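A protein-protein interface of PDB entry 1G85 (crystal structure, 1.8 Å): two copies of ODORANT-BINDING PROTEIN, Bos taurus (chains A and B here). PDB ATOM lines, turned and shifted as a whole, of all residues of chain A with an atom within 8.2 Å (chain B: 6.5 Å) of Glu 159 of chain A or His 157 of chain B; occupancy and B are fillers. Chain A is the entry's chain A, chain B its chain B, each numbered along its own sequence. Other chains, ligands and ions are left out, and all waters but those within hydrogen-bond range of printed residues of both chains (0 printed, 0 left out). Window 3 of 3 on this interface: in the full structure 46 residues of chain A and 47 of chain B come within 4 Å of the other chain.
The side-chain hydroxyl of Tyr 39 of chain A sits at hydrogen-bond distance from the side-chain amide nitrogen of Asn 152 of chain B. The backbone NH of His 157 of chain B lies within hydrogen-bond range of the backbone carbonyl oxygen of His 157 of chain A (3.5 Å). OXT of Glu 159 of chain A sits at hydrogen-bond distance from NE2 of His 157 of chain B (2.7 Å).
The guanidinium group (NH1) of Arg 37 of chain A lies within salt-bridge range of the side-chain carboxylate (OE2) of Glu 159 of chain A, 3.0 Å away. The backbone carbonyl oxygen (O) of Tyr 39 of chain A lies within hydrogen-bond range of the backbone NH (N) of Ser 57 of chain A (3.0 Å). The side-chain hydroxyl (OH) of Tyr 39 of chain A lies within hydrogen-bond range of the side-chain carboxylate (OE2) of Glu 159 of chain A. The side-chain amino group (NZ) of Lys 59 of chain A lies within salt-bridge range of the chain-end carboxylate (OXT) of Glu 159 of chain A (3.0 Å). The indole nitrogen of Trp 64 of chain A lies close to the chain-end carboxylate of Glu 159 of chain A. The backbone carbonyl oxygen (O) of Pro 156 of chain B lies within hydrogen-bond range of the side-chain amide nitrogen (ND2) of Asn 66 of chain B (2.8 Å).
Among the printed residues, merely in contact across the chains: His 157 of chain A with Pro 156 of chain B (3.1 Å), His 155 of chain A with Trp 64 of chain B (3.3 Å), Pro 156 of chain A with Trp 64 of chain B (3.4 Å), Arg 37 of chain A with Val 147 of chain B (3.5 Å), Tyr 39 of chain A with Phe 149 of chain B (3.5 Å), Arg 37 of chain A with Phe 149 of chain B (3.6 Å), Thr 38 of chain A with Phe 149 of chain B (3.7 Å), Pro 158 of chain A with Asn 152 of chain B (3.7 Å), Pro 156 of chain A with Ser 57 of chain B (3.9 Å), Arg 37 of chain A with Asn 152 of chain B (3.9 Å) and Ile 30 of chain A with Val 147 of chain B (3.9 Å).
Printed residues of chain B within 4 Å of Ile 30 of chain A: Val 147 (3.9 Å). Gln 31 of chain A touches none of the printed residues of chain B. Printed residues of chain B within 4 Å of Arg 37 of chain A: Val 147, Phe 149 and Asn 152. Of the printed residues of chain B, His 157 of chain A touches Pro 156 (3.1 Å) and His 157 (3.5 Å). Glu 159 of chain A touches one residue of chain B. Printed residues of chain A within 4 Å of Val 147 of chain B: Ile 30 and Arg 37. Of the printed residues of chain A, His 157 of chain B touches His 157 (3.5 Å) and Glu 159 (2.7 Å). The nearest printed residue of chain B that does not touch Pro 158 of chain A is Pro 156 of chain B (4.4 Å).
Hydrophobic or aromatic side chains of chain A within 4 Å of the printed part of chain B: Ile 30, Tyr 39 and Pro 156. Printed residues of chain B that touch a printed residue of chain A: Ser 57, Trp 64, Val 147, Phe 149, Asn 152, Pro 156 and His 157. Along chain B the printed residues that touch a printed residue of chain A span positions 57 to 157. Among the printed residues, 14 pairs touch across the chains. Among the printed residues, no Asp or Glu carboxylate lies within 4 Å of a Lys or Arg side-chain nitrogen of the other chain.
His 155 of chain A touches Trp 64 of chain B, but with the chains exchanged Trp 64 of chain A does not touch His 155 of chain B (10.4 Å). Pro 156 of chain A touches Ser 57 of chain B, but with the chains exchanged Ser 57 of chain A does not touch Pro 156 of chain B (12.7 Å). His 157 of chain A touches Pro 156 of chain B, but with the chains exchanged Pro 156 of chain A does not touch His 157 of chain B (5.6 Å). His 157 of chain A touches its own counterpart, His 157 of chain B. 5 positions are printed for both chains. Of the 14 pairs that touch across the chains among the printed residues, 1 has its exchanged pair printed and touching as well.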
ATOM      1  N   ILE A  30      -5.682  34.480  15.520  1.00  0.00           N
ATOM      2  CA  ILE A  30      -6.793  33.546  15.679  1.00  0.00           C
ATOM      3  C   ILE A  30      -8.176  34.163  15.518  1.00  0.00           C
ATOM      4  O   ILE A  30      -9.190  33.470  15.641  1.00  0.00           O
ATOM      5  CB  ILE A  30      -6.730  32.801  17.033  1.00  0.00           C
ATOM      6  CG1 ILE A  30      -6.748  33.794  18.193  1.00  0.00           C
ATOM      7  CG2 ILE A  30      -5.487  31.922  17.068  1.00  0.00           C
ATOM      8  CD1 ILE A  30      -6.815  33.139  19.556  1.00  0.00           C
ATOM      9  N   GLN A  31      -8.220  35.463  15.248  1.00  0.00           N
ATOM     10  CA  GLN A  31      -9.500  36.134  15.039  1.00  0.00           C
ATOM     11  C   GLN A  31     -10.045  35.667  13.698  1.00  0.00           C
ATOM     12  O   GLN A  31      -9.352  34.978  12.945  1.00  0.00           O
ATOM     13  CB  GLN A  31      -9.319  37.653  15.014  1.00  0.00           C
ATOM     14  CG  GLN A  31      -9.055  38.284  16.378  1.00  0.00           C
ATOM     15  CD  GLN A  31      -8.597  39.727  16.278  1.00  0.00           C
ATOM     16  OE1 GLN A  31      -8.397  40.395  17.292  1.00  0.00           O
ATOM     17  NE2 GLN A  31      -8.420  40.214  15.052  1.00  0.00           N
ATOM     18  N   GLU A  32     -11.283  36.036  13.397  1.00  0.00           N
ATOM     19  CA  GLU A  32     -11.887  35.644  12.133  1.00  0.00           C
ATOM     20  C   GLU A  32     -10.934  35.998  10.998  1.00  0.00           C
ATOM     21  O   GLU A  32     -10.366  37.088  10.970  1.00  0.00           O
ATOM     22  CB  GLU A  32     -13.230  36.352  11.951  1.00  0.00           C
ATOM     23  CG  GLU A  32     -14.181  36.140  13.134  1.00  0.00           C
ATOM     24  CD  GLU A  32     -15.589  35.789  12.702  1.00  0.00           C
ATOM     25  OE1 GLU A  32     -16.442  35.574  13.587  1.00  0.00           O
ATOM     26  OE2 GLU A  32     -15.843  35.723  11.480  1.00  0.00           O
ATOM     27  N   ASN A  33     -10.753  35.053  10.078  1.00  0.00           N
ATOM     28  CA  ASN A  33      -9.862  35.216   8.934  1.00  0.00           C
ATOM     29  C   ASN A  33      -8.399  35.036   9.344  1.00  0.00           C
ATOM     30  O   ASN A  33      -7.495  35.158   8.520  1.00  0.00           O
ATOM     31  CB  ASN A  33     -10.050  36.593   8.288  1.00  0.00           C
ATOM     32  CG  ASN A  33     -10.149  36.515   6.777  1.00  0.00           C
ATOM     33  OD1 ASN A  33      -9.642  37.382   6.062  1.00  0.00           O
ATOM     34  ND2 ASN A  33     -10.818  35.481   6.281  1.00  0.00           N
ATOM     35  N   GLY A  34      -8.172  34.742  10.620  1.00  0.00           N
ATOM     36  CA  GLY A  34      -6.816  34.547  11.101  1.00  0.00           C
ATOM     37  C   GLY A  34      -6.235  33.236  10.604  1.00  0.00           C
ATOM     38  O   GLY A  34      -6.963  32.259  10.461  1.00  0.00           O
ATOM     39  N   ARG A  37      -6.839  30.097  13.084  1.00  0.00           N
ATOM     40  CA  ARG A  37      -8.189  29.778  13.558  1.00  0.00           C
ATOM     41  C   ARG A  37      -8.487  28.458  12.846  1.00  0.00           C
ATOM     42  O   ARG A  37      -9.321  28.384  11.943  1.00  0.00           O
ATOM     43  CB  ARG A  37      -9.176  30.864  13.126  1.00  0.00           C
ATOM     44  CG  ARG A  37     -10.650  30.547  13.458  1.00  0.00           C
ATOM     45  CD  ARG A  37     -11.547  31.769  13.227  1.00  0.00           C
ATOM     46  NE  ARG A  37     -11.414  32.723  14.319  1.00  0.00           N
ATOM     47  CZ  ARG A  37     -12.344  32.936  15.243  1.00  0.00           C
ATOM     48  NH1 ARG A  37     -13.491  32.268  15.204  1.00  0.00           N
ATOM     49  NH2 ARG A  37     -12.116  33.797  16.220  1.00  0.00           N
ATOM     50  N   THR A  38      -7.795  27.413  13.286  1.00  0.00           N
ATOM     51  CA  THR A  38      -7.875  26.103  12.661  1.00  0.00           C
ATOM     52  C   THR A  38      -8.787  25.053  13.282  1.00  0.00           C
ATOM     53  O   THR A  38      -8.620  24.682  14.437  1.00  0.00           O
ATOM     54  CB  THR A  38      -6.468  25.493  12.573  1.00  0.00           C
ATOM     55  OG1 THR A  38      -5.943  25.341  13.899  1.00  0.00           O
ATOM     56  CG2 THR A  38      -5.537  26.408  11.787  1.00  0.00           C
ATOM     57  N   TYR A  39      -9.738  24.570  12.487  1.00  0.00           N
ATOM     58  CA  TYR A  39     -10.658  23.525  12.920  1.00  0.00           C
ATOM     59  C   TYR A  39     -10.073  22.176  12.491  1.00  0.00           C
ATOM     60  O   TYR A  39     -10.137  21.804  11.324  1.00  0.00           O
ATOM     61  CB  TYR A  39     -12.033  23.722  12.271  1.00  0.00           C
ATOM     62  CG  TYR A  39     -12.784  24.929  12.776  1.00  0.00           C
ATOM     63  CD1 TYR A  39     -13.675  24.822  13.845  1.00  0.00           C
ATOM     64  CD2 TYR A  39     -12.579  26.191  12.215  1.00  0.00           C
ATOM     65  CE1 TYR A  39     -14.344  25.941  14.344  1.00  0.00           C
ATOM     66  CE2 TYR A  39     -13.243  27.320  12.711  1.00  0.00           C
ATOM     67  CZ  TYR A  39     -14.122  27.182  13.776  1.00  0.00           C
ATOM     68  OH  TYR A  39     -14.774  28.282  14.282  1.00  0.00           O
ATOM     69  N   SER A  57      -9.183  22.633   8.657  1.00  0.00           N
ATOM     70  CA  SER A  57      -9.870  23.596   7.808  1.00  0.00           C
ATOM     71  C   SER A  57      -9.748  25.001   8.380  1.00  0.00           C
ATOM     72  O   SER A  57      -9.795  25.198   9.595  1.00  0.00           O
ATOM     73  CB  SER A  57     -11.353  23.242   7.692  1.00  0.00           C
ATOM     74  OG  SER A  57     -11.531  21.968   7.106  1.00  0.00           O
ATOM     75  N   VAL A  58      -9.590  25.973   7.493  1.00  0.00           N
ATOM     76  CA  VAL A  58      -9.484  27.370   7.884  1.00  0.00           C
ATOM     77  C   VAL A  58     -10.179  28.216   6.835  1.00  0.00           C
ATOM     78  O   VAL A  58     -10.181  27.872   5.655  1.00  0.00           O
ATOM     79  CB  VAL A  58      -8.013  27.839   8.008  1.00  0.00           C
ATOM     80  CG1 VAL A  58      -7.450  27.416   9.347  1.00  0.00           C
ATOM     81  CG2 VAL A  58      -7.173  27.261   6.878  1.00  0.00           C
ATOM     82  N   LYS A  59     -10.786  29.310   7.275  1.00  0.00           N
ATOM     83  CA  LYS A  59     -11.486  30.199   6.361  1.00  0.00           C
ATOM     84  C   LYS A  59     -10.551  31.351   6.019  1.00  0.00           C
ATOM     85  O   LYS A  59     -10.039  32.030   6.910  1.00  0.00           O
ATOM     86  CB  LYS A  59     -12.765  30.719   7.020  1.00  0.00           C
ATOM     87  CG  LYS A  59     -13.773  31.352   6.055  1.00  0.00           C
ATOM     88  CD  LYS A  59     -15.044  31.809   6.806  1.00  0.00           C
ATOM     89  CE  LYS A  59     -16.059  32.438   5.859  1.00  0.00           C
ATOM     90  NZ  LYS A  59     -17.287  32.893   6.572  1.00  0.00           N
ATOM     91  N   ARG A  60     -10.314  31.553   4.727  1.00  0.00           N
ATOM     92  CA  ARG A  60      -9.434  32.617   4.261  1.00  0.00           C
ATOM     93  C   ARG A  60     -10.104  33.456   3.180  1.00  0.00           C
ATOM     94  O   ARG A  60     -10.604  32.921   2.191  1.00  0.00           O
ATOM     95  CB  ARG A  60      -8.142  32.034   3.682  1.00  0.00           C
ATOM     96  CG  ARG A  60      -7.268  31.260   4.659  1.00  0.00           C
ATOM     97  CD  ARG A  60      -6.788  32.135   5.817  1.00  0.00           C
ATOM     98  NE  ARG A  60      -5.602  31.566   6.451  1.00  0.00           N
ATOM     99  CZ  ARG A  60      -4.360  31.985   6.229  1.00  0.00           C
ATOM    100  NH1 ARG A  60      -4.131  32.990   5.393  1.00  0.00           N
ATOM    101  NH2 ARG A  60      -3.343  31.386   6.829  1.00  0.00           N
ATOM    102  N   GLY A  62     -12.888  34.853   3.044  1.00  0.00           N
ATOM    103  CA  GLY A  62     -14.266  34.463   2.824  1.00  0.00           C
ATOM    104  C   GLY A  62     -14.456  33.111   2.160  1.00  0.00           C
ATOM    105  O   GLY A  62     -15.553  32.801   1.691  1.00  0.00           O
ATOM    106  N   TRP A  64     -13.507  28.729   2.442  1.00  0.00           N
ATOM    107  CA  TRP A  64     -13.012  27.637   3.272  1.00  0.00           C
ATOM    108  C   TRP A  64     -11.939  26.835   2.556  1.00  0.00           C
ATOM    109  O   TRP A  64     -12.072  26.508   1.377  1.00  0.00           O
ATOM    110  CB  TRP A  64     -14.148  26.708   3.700  1.00  0.00           C
ATOM    111  CG  TRP A  64     -14.944  27.266   4.826  1.00  0.00           C
ATOM    112  CD1 TRP A  64     -16.117  27.949   4.742  1.00  0.00           C
ATOM    113  CD2 TRP A  64     -14.588  27.237   6.216  1.00  0.00           C
ATOM    114  NE1 TRP A  64     -16.521  28.349   5.995  1.00  0.00           N
ATOM    115  CE2 TRP A  64     -15.604  27.924   6.914  1.00  0.00           C
ATOM    116  CE3 TRP A  64     -13.514  26.695   6.932  1.00  0.00           C
ATOM    117  CZ2 TRP A  64     -15.570  28.088   8.305  1.00  0.00           C
ATOM    118  CZ3 TRP A  64     -13.481  26.858   8.312  1.00  0.00           C
ATOM    119  CH2 TRP A  64     -14.507  27.548   8.984  1.00  0.00           C
ATOM    120  N   HIS A 155     -20.181  19.170   4.569  1.00  0.00           N
ATOM    121  CA  HIS A 155     -20.478  19.348   5.992  1.00  0.00           C
ATOM    122  C   HIS A 155     -20.769  20.809   6.362  1.00  0.00           C
ATOM    123  O   HIS A 155     -20.407  21.727   5.628  1.00  0.00           O
ATOM    124  CB  HIS A 155     -19.311  18.814   6.831  1.00  0.00           C
ATOM    125  CG  HIS A 155     -17.994  19.456   6.519  1.00  0.00           C
ATOM    126  ND1 HIS A 155     -17.706  20.766   6.845  1.00  0.00           N
ATOM    127  CD2 HIS A 155     -16.887  18.970   5.909  1.00  0.00           C
ATOM    128  CE1 HIS A 155     -16.480  21.056   6.451  1.00  0.00           C
ATOM    129  NE2 HIS A 155     -15.961  19.984   5.880  1.00  0.00           N
ATOM    130  N   PRO A 156     -21.435  21.039   7.512  1.00  0.00           N
ATOM    131  CA  PRO A 156     -21.781  22.387   7.985  1.00  0.00           C
ATOM    132  C   PRO A 156     -20.557  23.258   8.270  1.00  0.00           C
ATOM    133  O   PRO A 156     -19.467  22.745   8.521  1.00  0.00           O
ATOM    134  CB  PRO A 156     -22.587  22.117   9.259  1.00  0.00           C
ATOM    135  CG  PRO A 156     -23.152  20.747   9.037  1.00  0.00           C
ATOM    136  CD  PRO A 156     -21.994  20.017   8.414  1.00  0.00           C
ATOM    137  N   HIS A 157     -20.748  24.574   8.238  1.00  0.00           N
ATOM    138  CA  HIS A 157     -19.664  25.520   8.504  1.00  0.00           C
ATOM    139  C   HIS A 157     -19.790  26.112   9.899  1.00  0.00           C
ATOM    140  O   HIS A 157     -20.858  26.574  10.292  1.00  0.00           O
ATOM    141  CB  HIS A 157     -19.678  26.662   7.487  1.00  0.00           C
ATOM    142  CG  HIS A 157     -19.574  26.205   6.067  1.00  0.00           C
ATOM    143  ND1 HIS A 157     -18.527  25.437   5.610  1.00  0.00           N
ATOM    144  CD2 HIS A 157     -20.392  26.401   5.007  1.00  0.00           C
ATOM    145  CE1 HIS A 157     -18.703  25.177   4.327  1.00  0.00           C
ATOM    146  NE2 HIS A 157     -19.827  25.750   3.936  1.00  0.00           N
ATOM    147  N   PRO A 158     -18.690  26.108  10.666  1.00  0.00           N
ATOM    148  CA  PRO A 158     -18.673  26.649  12.030  1.00  0.00           C
ATOM    149  C   PRO A 158     -18.802  28.169  12.050  1.00  0.00           C
ATOM    150  O   PRO A 158     -19.158  28.759  13.071  1.00  0.00           O
ATOM    151  CB  PRO A 158     -17.316  26.194  12.567  1.00  0.00           C
ATOM    152  CG  PRO A 158     -17.013  24.962  11.763  1.00  0.00           C
ATOM    153  CD  PRO A 158     -17.445  25.372  10.384  1.00  0.00           C
ATOM    154  N   GLU A 159     -18.508  28.796  10.916  1.00  0.00           N
ATOM    155  CA  GLU A 159     -18.565  30.248  10.804  1.00  0.00           C
ATOM    156  C   GLU A 159     -18.575  30.690   9.344  1.00  0.00           C
ATOM    157  O   GLU A 159     -18.488  29.809   8.464  1.00  0.00           O
ATOM    158  CB  GLU A 159     -17.363  30.870  11.524  1.00  0.00           C
ATOM    159  CG  GLU A 159     -16.057  30.102  11.312  1.00  0.00           C
ATOM    160  CD  GLU A 159     -14.862  30.775  11.961  1.00  0.00           C
ATOM    161  OE1 GLU A 159     -14.296  31.708  11.354  1.00  0.00           O
ATOM    162  OE2 GLU A 159     -14.493  30.379  13.084  1.00  0.00           O
ATOM    163  OXT GLU A 159     -18.668  31.914   9.102  1.00  0.00           O
ATOM    164  N   SER B  57     -27.891  19.749  12.243  1.00  0.00           N
ATOM    165  CA  SER B  57     -27.877  20.578  11.052  1.00  0.00           C
ATOM    166  C   SER B  57     -28.130  19.680   9.859  1.00  0.00           C
ATOM    167  O   SER B  57     -27.658  18.538   9.802  1.00  0.00           O
ATOM    168  CB  SER B  57     -26.524  21.274  10.893  1.00  0.00           C
ATOM    169  OG  SER B  57     -26.279  22.170  11.964  1.00  0.00           O
ATOM    170  N   TRP B  64     -27.557  25.065   4.608  1.00  0.00           N
ATOM    171  CA  TRP B  64     -27.553  24.418   5.910  1.00  0.00           C
ATOM    172  C   TRP B  64     -28.540  25.069   6.862  1.00  0.00           C
ATOM    173  O   TRP B  64     -28.606  26.294   6.966  1.00  0.00           O
ATOM    174  CB  TRP B  64     -26.150  24.469   6.508  1.00  0.00           C
ATOM    175  CG  TRP B  64     -25.210  23.545   5.824  1.00  0.00           C
ATOM    176  CD1 TRP B  64     -24.262  23.866   4.892  1.00  0.00           C
ATOM    177  CD2 TRP B  64     -25.147  22.131   5.994  1.00  0.00           C
ATOM    178  NE1 TRP B  64     -23.608  22.731   4.476  1.00  0.00           N
ATOM    179  CE2 TRP B  64     -24.131  21.650   5.142  1.00  0.00           C
ATOM    180  CE3 TRP B  64     -25.847  21.219   6.797  1.00  0.00           C
ATOM    181  CZ2 TRP B  64     -23.804  20.295   5.057  1.00  0.00           C
ATOM    182  CZ3 TRP B  64     -25.523  19.873   6.716  1.00  0.00           C
ATOM    183  CH2 TRP B  64     -24.505  19.424   5.855  1.00  0.00           C
ATOM    184  N   ASN B  66     -30.261  24.904  10.915  1.00  0.00           N
ATOM    185  CA  ASN B  66     -30.098  24.394  12.270  1.00  0.00           C
ATOM    186  C   ASN B  66     -31.496  24.001  12.726  1.00  0.00           C
ATOM    187  O   ASN B  66     -32.426  24.807  12.669  1.00  0.00           O
ATOM    188  CB  ASN B  66     -29.515  25.456  13.199  1.00  0.00           C
ATOM    189  CG  ASN B  66     -28.061  25.762  12.893  1.00  0.00           C
ATOM    190  OD1 ASN B  66     -27.320  24.894  12.436  1.00  0.00           O
ATOM    191  ND2 ASN B  66     -27.644  26.995  13.160  1.00  0.00           N
ATOM    192  N   VAL B 147     -10.096  31.377  21.841  1.00  0.00           N
ATOM    193  CA  VAL B 147     -11.304  31.086  21.084  1.00  0.00           C
ATOM    194  C   VAL B 147     -11.822  29.684  21.387  1.00  0.00           C
ATOM    195  O   VAL B 147     -11.046  28.725  21.453  1.00  0.00           O
ATOM    196  CB  VAL B 147     -11.038  31.192  19.568  1.00  0.00           C
ATOM    197  CG1 VAL B 147     -12.264  30.731  18.784  1.00  0.00           C
ATOM    198  CG2 VAL B 147     -10.679  32.620  19.207  1.00  0.00           C
ATOM    199  N   PHE B 149     -13.572  26.863  19.917  1.00  0.00           N
ATOM    200  CA  PHE B 149     -13.953  26.276  18.639  1.00  0.00           C
ATOM    201  C   PHE B 149     -15.106  25.295  18.767  1.00  0.00           C
ATOM    202  O   PHE B 149     -15.942  25.190  17.871  1.00  0.00           O
ATOM    203  CB  PHE B 149     -12.751  25.572  17.997  1.00  0.00           C
ATOM    204  CG  PHE B 149     -11.674  26.524  17.553  1.00  0.00           C
ATOM    205  CD1 PHE B 149     -10.886  27.194  18.486  1.00  0.00           C
ATOM    206  CD2 PHE B 149     -11.450  26.755  16.200  1.00  0.00           C
ATOM    207  CE1 PHE B 149      -9.917  28.107  18.077  1.00  0.00           C
ATOM    208  CE2 PHE B 149     -10.482  27.667  15.785  1.00  0.00           C
ATOM    209  CZ  PHE B 149      -9.709  28.331  16.724  1.00  0.00           C
ATOM    210  N   ASN B 152     -18.425  26.913  18.601  1.00  0.00           N
ATOM    211  CA  ASN B 152     -18.720  27.435  17.265  1.00  0.00           C
ATOM    212  C   ASN B 152     -19.296  26.291  16.429  1.00  0.00           C
ATOM    213  O   ASN B 152     -20.294  26.464  15.720  1.00  0.00           O
ATOM    214  CB  ASN B 152     -17.463  27.992  16.586  1.00  0.00           C
ATOM    215  CG  ASN B 152     -16.993  29.297  17.200  1.00  0.00           C
ATOM    216  OD1 ASN B 152     -17.770  30.017  17.828  1.00  0.00           O
ATOM    217  ND2 ASN B 152     -15.720  29.617  17.002  1.00  0.00           N
ATOM    218  N   HIS B 155     -22.843  25.484  17.288  1.00  0.00           N
ATOM    219  CA  HIS B 155     -23.827  26.489  16.900  1.00  0.00           C
ATOM    220  C   HIS B 155     -23.399  27.096  15.569  1.00  0.00           C
ATOM    221  O   HIS B 155     -23.028  28.262  15.509  1.00  0.00           O
ATOM    222  CB  HIS B 155     -23.916  27.594  17.956  1.00  0.00           C
ATOM    223  CG  HIS B 155     -24.077  27.089  19.355  1.00  0.00           C
ATOM    224  ND1 HIS B 155     -23.018  26.620  20.106  1.00  0.00           N
ATOM    225  CD2 HIS B 155     -25.167  26.998  20.153  1.00  0.00           C
ATOM    226  CE1 HIS B 155     -23.449  26.267  21.301  1.00  0.00           C
ATOM    227  NE2 HIS B 155     -24.753  26.486  21.358  1.00  0.00           N
ATOM    228  N   PRO B 156     -23.444  26.306  14.487  1.00  0.00           N
ATOM    229  CA  PRO B 156     -23.053  26.763  13.150  1.00  0.00           C
ATOM    230  C   PRO B 156     -24.082  27.680  12.506  1.00  0.00           C
ATOM    231  O   PRO B 156     -25.084  28.033  13.120  1.00  0.00           O
ATOM    232  CB  PRO B 156     -22.908  25.458  12.380  1.00  0.00           C
ATOM    233  CG  PRO B 156     -24.027  24.644  12.944  1.00  0.00           C
ATOM    234  CD  PRO B 156     -23.895  24.902  14.441  1.00  0.00           C
ATOM    235  N   HIS B 157     -23.824  28.070  11.261  1.00  0.00           N
ATOM    236  CA  HIS B 157     -24.755  28.924  10.534  1.00  0.00           C
ATOM    237  C   HIS B 157     -24.651  28.688   9.034  1.00  0.00           C
ATOM    238  O   HIS B 157     -23.816  27.853   8.630  1.00  0.00           O
ATOM    239  CB  HIS B 157     -24.507  30.403  10.858  1.00  0.00           C
ATOM    240  CG  HIS B 157     -23.209  30.936  10.339  1.00  0.00           C
ATOM    241  ND1 HIS B 157     -22.865  30.889   9.005  1.00  0.00           N
ATOM    242  CD2 HIS B 157     -22.190  31.567  10.968  1.00  0.00           C
ATOM    243  CE1 HIS B 157     -21.690  31.471   8.834  1.00  0.00           C
ATOM    244  NE2 HIS B 157     -21.260  31.891  10.010  1.00  0.00           N
